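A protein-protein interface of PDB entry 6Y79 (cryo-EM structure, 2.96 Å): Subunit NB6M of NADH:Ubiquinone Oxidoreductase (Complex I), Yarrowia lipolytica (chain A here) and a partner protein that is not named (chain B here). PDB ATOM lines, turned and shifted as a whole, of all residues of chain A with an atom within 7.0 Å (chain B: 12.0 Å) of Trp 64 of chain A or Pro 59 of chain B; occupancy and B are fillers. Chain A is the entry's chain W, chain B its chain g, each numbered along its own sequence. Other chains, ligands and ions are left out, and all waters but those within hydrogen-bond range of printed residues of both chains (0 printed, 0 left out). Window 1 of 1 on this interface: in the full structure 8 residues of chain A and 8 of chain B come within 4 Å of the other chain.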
ATOM      1  N   LYS A  59      27.591 -31.443 -25.255  1.00  0.00           N
ATOM      2  CA  LYS A  59      26.524 -30.921 -26.102  1.00  0.00           C
ATOM      3  C   LYS A  59      26.725 -29.445 -26.392  1.00  0.00           C
ATOM      4  O   LYS A  59      26.458 -28.991 -27.511  1.00  0.00           O
ATOM      5  CB  LYS A  59      25.170 -31.143 -25.439  1.00  0.00           C
ATOM      6  CG  LYS A  59      23.989 -30.749 -26.288  1.00  0.00           C
ATOM      7  CD  LYS A  59      23.956 -31.539 -27.571  1.00  0.00           C
ATOM      8  CE  LYS A  59      22.777 -31.130 -28.415  1.00  0.00           C
ATOM      9  NZ  LYS A  59      21.523 -31.091 -27.627  1.00  0.00           N
ATOM     10  N   ARG A  60      27.201 -28.690 -25.395  1.00  0.00           N
ATOM     11  CA  ARG A  60      27.549 -27.286 -25.613  1.00  0.00           C
ATOM     12  C   ARG A  60      28.606 -27.136 -26.698  1.00  0.00           C
ATOM     13  O   ARG A  60      28.471 -26.294 -27.598  1.00  0.00           O
ATOM     14  CB  ARG A  60      28.042 -26.653 -24.317  1.00  0.00           C
ATOM     15  CG  ARG A  60      28.503 -25.229 -24.490  1.00  0.00           C
ATOM     16  CD  ARG A  60      28.873 -24.613 -23.173  1.00  0.00           C
ATOM     17  NE  ARG A  60      27.729 -24.573 -22.275  1.00  0.00           N
ATOM     18  CZ  ARG A  60      27.795 -24.183 -21.012  1.00  0.00           C
ATOM     19  NH1 ARG A  60      26.714 -24.182 -20.258  1.00  0.00           N
ATOM     20  NH2 ARG A  60      28.946 -23.796 -20.500  1.00  0.00           N
ATOM     21  N   GLU A  61      29.637 -27.984 -26.652  1.00  0.00           N
ATOM     22  CA  GLU A  61      30.695 -27.946 -27.664  1.00  0.00           C
ATOM     23  C   GLU A  61      30.158 -28.214 -29.073  1.00  0.00           C
ATOM     24  O   GLU A  61      30.404 -27.429 -30.003  1.00  0.00           O
ATOM     25  CB  GLU A  61      31.782 -28.954 -27.311  1.00  0.00           C
ATOM     26  CG  GLU A  61      33.114 -28.667 -27.954  1.00  0.00           C
ATOM     27  CD  GLU A  61      34.078 -29.813 -27.822  1.00  0.00           C
ATOM     28  OE1 GLU A  61      33.710 -30.826 -27.196  1.00  0.00           O
ATOM     29  OE2 GLU A  61      35.205 -29.704 -28.343  1.00  0.00           O
ATOM     30  N   LYS A  62      29.388 -29.298 -29.239  1.00  0.00           N
ATOM     31  CA  LYS A  62      28.835 -29.637 -30.559  1.00  0.00           C
ATOM     32  C   LYS A  62      27.864 -28.572 -31.062  1.00  0.00           C
ATOM     33  O   LYS A  62      27.788 -28.288 -32.269  1.00  0.00           O
ATOM     34  CB  LYS A  62      28.132 -30.989 -30.485  1.00  0.00           C
ATOM     35  CG  LYS A  62      27.550 -31.458 -31.790  1.00  0.00           C
ATOM     36  CD  LYS A  62      26.930 -32.821 -31.658  1.00  0.00           C
ATOM     37  CE  LYS A  62      25.569 -32.745 -31.024  1.00  0.00           C
ATOM     38  NZ  LYS A  62      24.934 -34.087 -31.018  1.00  0.00           N
ATOM     39  N   LEU A  63      27.185 -27.917 -30.127  1.00  0.00           N
ATOM     40  CA  LEU A  63      26.201 -26.895 -30.436  1.00  0.00           C
ATOM     41  C   LEU A  63      26.856 -25.646 -31.017  1.00  0.00           C
ATOM     42  O   LEU A  63      26.412 -25.118 -32.052  1.00  0.00           O
ATOM     43  CB  LEU A  63      25.474 -26.597 -29.139  1.00  0.00           C
ATOM     44  CG  LEU A  63      24.193 -25.877 -28.974  1.00  0.00           C
ATOM     45  CD1 LEU A  63      23.162 -26.679 -29.732  1.00  0.00           C
ATOM     46  CD2 LEU A  63      23.992 -25.987 -27.515  1.00  0.00           C
ATOM     47  N   TRP A  64      27.917 -25.156 -30.358  1.00  0.00           N
ATOM     48  CA  TRP A  64      28.646 -24.009 -30.900  1.00  0.00           C
ATOM     49  C   TRP A  64      29.327 -24.348 -32.223  1.00  0.00           C
ATOM     50  O   TRP A  64      29.443 -23.475 -33.092  1.00  0.00           O
ATOM     51  CB  TRP A  64      29.667 -23.477 -29.889  1.00  0.00           C
ATOM     52  CG  TRP A  64      29.050 -22.806 -28.687  1.00  0.00           C
ATOM     53  CD1 TRP A  64      28.884 -23.341 -27.457  1.00  0.00           C
ATOM     54  CD2 TRP A  64      28.533 -21.475 -28.607  1.00  0.00           C
ATOM     55  NE1 TRP A  64      28.284 -22.448 -26.615  1.00  0.00           N
ATOM     56  CE2 TRP A  64      28.062 -21.287 -27.300  1.00  0.00           C
ATOM     57  CE3 TRP A  64      28.443 -20.421 -29.507  1.00  0.00           C
ATOM     58  CZ2 TRP A  64      27.490 -20.095 -26.881  1.00  0.00           C
ATOM     59  CZ3 TRP A  64      27.851 -19.250 -29.101  1.00  0.00           C
ATOM     60  CH2 TRP A  64      27.397 -19.089 -27.796  1.00  0.00           C
ATOM     61  N   ALA A  65      29.721 -25.614 -32.421  1.00  0.00           N
ATOM     62  CA  ALA A  65      30.238 -26.030 -33.727  1.00  0.00           C
ATOM     63  C   ALA A  65      29.185 -25.910 -34.828  1.00  0.00           C
ATOM     64  O   ALA A  65      29.470 -25.403 -35.924  1.00  0.00           O
ATOM     65  CB  ALA A  65      30.749 -27.465 -33.650  1.00  0.00           C
ATOM     66  N   ARG A  66      27.956 -26.350 -34.546  1.00  0.00           N
ATOM     67  CA  ARG A  66      26.905 -26.298 -35.562  1.00  0.00           C
ATOM     68  C   ARG A  66      26.498 -24.868 -35.888  1.00  0.00           C
ATOM     69  O   ARG A  66      26.191 -24.554 -37.045  1.00  0.00           O
ATOM     70  CB  ARG A  66      25.690 -27.095 -35.109  1.00  0.00           C
ATOM     71  CG  ARG A  66      25.881 -28.569 -35.197  1.00  0.00           C
ATOM     72  CD  ARG A  66      24.638 -29.287 -34.794  1.00  0.00           C
ATOM     73  NE  ARG A  66      24.862 -30.720 -34.791  1.00  0.00           N
ATOM     74  CZ  ARG A  66      23.930 -31.616 -34.511  1.00  0.00           C
ATOM     75  NH1 ARG A  66      24.228 -32.904 -34.532  1.00  0.00           N
ATOM     76  NH2 ARG A  66      22.703 -31.225 -34.209  1.00  0.00           N
ATOM     77  N   ILE A  67      26.498 -23.976 -34.898  1.00  0.00           N
ATOM     78  CA  ILE A  67      26.143 -22.608 -35.265  1.00  0.00           C
ATOM     79  C   ILE A  67      27.305 -21.854 -35.878  1.00  0.00           C
ATOM     80  O   ILE A  67      27.089 -20.813 -36.505  1.00  0.00           O
ATOM     81  CB  ILE A  67      25.582 -21.799 -34.094  1.00  0.00           C
ATOM     82  CG1 ILE A  67      26.600 -21.672 -32.995  1.00  0.00           C
ATOM     83  CG2 ILE A  67      24.352 -22.433 -33.590  1.00  0.00           C
ATOM     84  CD1 ILE A  67      26.071 -20.874 -31.923  1.00  0.00           C
ATOM     85  N   TYR A  68      28.538 -22.327 -35.709  1.00  0.00           N
ATOM     86  CA  TYR A  68      29.602 -21.799 -36.554  1.00  0.00           C
ATOM     87  C   TYR A  68      29.440 -22.260 -37.993  1.00  0.00           C
ATOM     88  O   TYR A  68      29.826 -21.543 -38.920  1.00  0.00           O
ATOM     89  CB  TYR A  68      30.964 -22.221 -36.024  1.00  0.00           C
ATOM     90  CG  TYR A  68      31.378 -21.526 -34.760  1.00  0.00           C
ATOM     91  CD1 TYR A  68      30.885 -20.274 -34.438  1.00  0.00           C
ATOM     92  CD2 TYR A  68      32.263 -22.130 -33.884  1.00  0.00           C
ATOM     93  CE1 TYR A  68      31.268 -19.640 -33.276  1.00  0.00           C
ATOM     94  CE2 TYR A  68      32.653 -21.506 -32.724  1.00  0.00           C
ATOM     95  CZ  TYR A  68      32.153 -20.262 -32.426  1.00  0.00           C
ATOM     96  OH  TYR A  68      32.541 -19.640 -31.269  1.00  0.00           O
ATOM     97  N   LEU A  69      28.877 -23.447 -38.199  1.00  0.00           N
ATOM     98  CA  LEU A  69      28.682 -23.936 -39.560  1.00  0.00           C
ATOM     99  C   LEU A  69      27.423 -23.416 -40.241  1.00  0.00           C
ATOM    100  O   LEU A  69      27.320 -23.551 -41.462  1.00  0.00           O
ATOM    101  CB  LEU A  69      28.625 -25.457 -39.578  1.00  0.00           C
ATOM    102  CG  LEU A  69      29.900 -26.158 -39.149  1.00  0.00           C
ATOM    103  CD1 LEU A  69      29.730 -27.660 -39.240  1.00  0.00           C
ATOM    104  CD2 LEU A  69      31.039 -25.669 -40.003  1.00  0.00           C
ATOM    105  N   HIS B  55      25.257 -23.866 -14.484  1.00  0.00           N
ATOM    106  CA  HIS B  55      25.858 -23.787 -15.801  1.00  0.00           C
ATOM    107  C   HIS B  55      25.204 -22.678 -16.615  1.00  0.00           C
ATOM    108  O   HIS B  55      24.078 -22.252 -16.349  1.00  0.00           O
ATOM    109  CB  HIS B  55      25.750 -25.130 -16.524  1.00  0.00           C
ATOM    110  CG  HIS B  55      24.350 -25.530 -16.875  1.00  0.00           C
ATOM    111  ND1 HIS B  55      23.447 -25.974 -15.937  1.00  0.00           N
ATOM    112  CD2 HIS B  55      23.709 -25.575 -18.065  1.00  0.00           C
ATOM    113  CE1 HIS B  55      22.305 -26.263 -16.532  1.00  0.00           C
ATOM    114  NE2 HIS B  55      22.437 -26.029 -17.823  1.00  0.00           N
ATOM    115  N   SER B  56      25.934 -22.200 -17.598  1.00  0.00           N
ATOM    116  CA  SER B  56      25.428 -21.184 -18.499  1.00  0.00           C
ATOM    117  C   SER B  56      24.537 -21.832 -19.560  1.00  0.00           C
ATOM    118  O   SER B  56      24.727 -23.002 -19.896  1.00  0.00           O
ATOM    119  CB  SER B  56      26.596 -20.445 -19.143  1.00  0.00           C
ATOM    120  OG  SER B  56      27.326 -19.733 -18.160  1.00  0.00           O
ATOM    121  N   PRO B  57      23.537 -21.114 -20.077  1.00  0.00           N
ATOM    122  CA  PRO B  57      22.568 -21.759 -20.967  1.00  0.00           C
ATOM    123  C   PRO B  57      23.142 -22.126 -22.322  1.00  0.00           C
ATOM    124  O   PRO B  57      23.994 -21.438 -22.886  1.00  0.00           O
ATOM    125  CB  PRO B  57      21.464 -20.705 -21.115  1.00  0.00           C
ATOM    126  CG  PRO B  57      22.122 -19.429 -20.787  1.00  0.00           C
ATOM    127  CD  PRO B  57      23.100 -19.758 -19.714  1.00  0.00           C
ATOM    128  N   LEU B  58      22.661 -23.244 -22.824  1.00  0.00           N
ATOM    129  CA  LEU B  58      22.981 -23.672 -24.166  1.00  0.00           C
ATOM    130  C   LEU B  58      22.286 -22.766 -25.181  1.00  0.00           C
ATOM    131  O   LEU B  58      21.157 -22.329 -24.948  1.00  0.00           O
ATOM    132  CB  LEU B  58      22.520 -25.112 -24.353  1.00  0.00           C
ATOM    133  CG  LEU B  58      23.057 -26.222 -23.450  1.00  0.00           C
ATOM    134  CD1 LEU B  58      22.724 -27.579 -24.039  1.00  0.00           C
ATOM    135  CD2 LEU B  58      24.533 -26.098 -23.256  1.00  0.00           C
ATOM    136  N   PRO B  59      22.930 -22.446 -26.301  1.00  0.00           N
ATOM    137  CA  PRO B  59      22.205 -21.786 -27.386  1.00  0.00           C
ATOM    138  C   PRO B  59      21.232 -22.740 -28.063  1.00  0.00           C
ATOM    139  O   PRO B  59      21.401 -23.958 -28.059  1.00  0.00           O
ATOM    140  CB  PRO B  59      23.319 -21.337 -28.335  1.00  0.00           C
ATOM    141  CG  PRO B  59      24.489 -22.203 -27.988  1.00  0.00           C
ATOM    142  CD  PRO B  59      24.383 -22.407 -26.518  1.00  0.00           C
ATOM    143  N   GLN B  60      20.179 -22.158 -28.622  1.00  0.00           N
ATOM    144  CA  GLN B  60      19.107 -22.893 -29.274  1.00  0.00           C
ATOM    145  C   GLN B  60      18.921 -22.529 -30.733  1.00  0.00           C
ATOM    146  O   GLN B  60      18.481 -23.370 -31.516  1.00  0.00           O
ATOM    147  CB  GLN B  60      17.787 -22.657 -28.544  1.00  0.00           C
ATOM    148  CG  GLN B  60      17.731 -23.273 -27.180  1.00  0.00           C
ATOM    149  CD  GLN B  60      16.568 -22.744 -26.386  1.00  0.00           C
ATOM    150  OE1 GLN B  60      15.913 -21.787 -26.795  1.00  0.00           O
ATOM    151  NE2 GLN B  60      16.296 -23.362 -25.250  1.00  0.00           N
ATOM    152  N   SER B  61      19.263 -21.310 -31.121  1.00  0.00           N
ATOM    153  CA  SER B  61      19.157 -20.874 -32.498  1.00  0.00           C
ATOM    154  C   SER B  61      20.521 -20.376 -32.940  1.00  0.00           C
ATOM    155  O   SER B  61      21.505 -20.573 -32.226  1.00  0.00           O
ATOM    156  CB  SER B  61      18.111 -19.775 -32.614  1.00  0.00           C
ATOM    157  OG  SER B  61      18.513 -18.645 -31.859  1.00  0.00           O
ATOM    158  N   TYR B  62      20.612 -19.751 -34.098  1.00  0.00           N
ATOM    159  CA  TYR B  62      21.771 -18.915 -34.340  1.00  0.00           C
ATOM    160  C   TYR B  62      21.659 -17.688 -33.444  1.00  0.00           C
ATOM    161  O   TYR B  62      20.594 -17.064 -33.390  1.00  0.00           O
ATOM    162  CB  TYR B  62      21.888 -18.484 -35.797  1.00  0.00           C
ATOM    163  CG  TYR B  62      23.160 -17.713 -36.062  1.00  0.00           C
ATOM    164  CD1 TYR B  62      24.363 -18.373 -36.269  1.00  0.00           C
ATOM    165  CD2 TYR B  62      23.163 -16.325 -36.085  1.00  0.00           C
ATOM    166  CE1 TYR B  62      25.526 -17.671 -36.499  1.00  0.00           C
ATOM    167  CE2 TYR B  62      24.319 -15.619 -36.300  1.00  0.00           C
ATOM    168  CZ  TYR B  62      25.495 -16.295 -36.514  1.00  0.00           C
ATOM    169  OH  TYR B  62      26.649 -15.591 -36.743  1.00  0.00           O
ATOM    170  N   PRO B  63      22.711 -17.314 -32.739  1.00  0.00           N
ATOM    171  CA  PRO B  63      22.654 -16.104 -31.918  1.00  0.00           C
ATOM    172  C   PRO B  63      22.744 -14.832 -32.745  1.00  0.00           C
ATOM    173  O   PRO B  63      23.809 -14.482 -33.264  1.00  0.00           O
ATOM    174  CB  PRO B  63      23.861 -16.261 -30.986  1.00  0.00           C
ATOM    175  CG  PRO B  63      24.796 -17.140 -31.716  1.00  0.00           C
ATOM    176  CD  PRO B  63      23.986 -18.026 -32.596  1.00  0.00           C
ATOM    177  N   LEU B  64      21.632 -14.141 -32.885  1.00  0.00           N
ATOM    178  CA  LEU B  64      21.659 -12.841 -33.542  1.00  0.00           C
ATOM    179  C   LEU B  64      22.042 -11.770 -32.537  1.00  0.00           C
ATOM    180  O   LEU B  64      21.401 -11.662 -31.488  1.00  0.00           O
ATOM    181  CB  LEU B  64      20.302 -12.493 -34.129  1.00  0.00           C
ATOM    182  CG  LEU B  64      19.756 -13.263 -35.320  1.00  0.00           C
ATOM    183  CD1 LEU B  64      18.322 -12.841 -35.557  1.00  0.00           C
ATOM    184  CD2 LEU B  64      20.599 -12.980 -36.531  1.00  0.00           C
ATOM    185  N   PRO B  65      23.065 -10.967 -32.803  1.00  0.00           N
ATOM    186  CA  PRO B  65      23.254  -9.754 -32.001  1.00  0.00           C
ATOM    187  C   PRO B  65      22.398  -8.625 -32.550  1.00  0.00           C
ATOM    188  O   PRO B  65      21.682  -8.817 -33.536  1.00  0.00           O
ATOM    189  CB  PRO B  65      24.752  -9.473 -32.136  1.00  0.00           C
ATOM    190  CG  PRO B  65      25.108 -10.038 -33.466  1.00  0.00           C
ATOM    191  CD  PRO B  65      24.195 -11.209 -33.719  1.00  0.00           C
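O of Ser 56 of chain B lies close to NH1 of Arg 60 of chain A, 2.3 Å away.
Among the printed residues, pairs that only touch across the chains: Arg 60 of chain A with His 55 of chain B, Arg 60 of chain A with Leu 58 of chain B, Leu 63 of chain A with Leu 58 of chain B, Leu 63 of chain A with Pro 59 of chain B, Trp 64 of chain A with Pro 59 of chain B, Ile 67 of chain A with Ser 61 of chain B, Ile 67 of chain A with Tyr 62 of chain B and Ile 67 of chain A with Pro 63 of chain B.
Printed residues of chain B within 4 Å of Trp 64 of chain A: Pro 59 (3.8 Å).
No residue of chain B comes within 4 Å of Ala 65 of chain A.
No residue of chain B comes within 4 Å of Tyr 68 of chain A.
Of the printed residues of chain A, His 55 of chain B touches Arg 60 (3.97 Å).
Printed residues of chain A within 4 Å of Ser 56 of chain B: Arg 60 (2.3 Å).
Printed residues of chain A within 4 Å of Pro 63 of chain B: Ile 67 (3.6 Å).
Of the printed residues of chain A, Leu 58 of chain B touches Arg 60 (3.7 Å) and Leu 63 (3.6 Å).
Of the printed residues of chain A, Tyr 62 of chain B touches Ile 67 (3.5 Å).
The nearest residue of chain B that does not touch Trp 64 of chain A is Pro 63 of chain B (4.5 Å).
The nearest printed residue of chain A that does not touch His 55 of chain B is Lys 59 of chain A (9.4 Å).
Of the 11 printed residues of chain A, 4 touch a printed residue of chain B.
Hydrophobic or aromatic side chains of chain A within 4 Å of the printed part of chain B: Leu 63, Trp 64 and Ile 67.
Hydrophobic or aromatic side chains of chain B that line the printed part of chain A: His 55, Leu 58, Pro 59, Tyr 62 and Pro 63.
Among the printed residues, 9 pairs touch across the chains.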
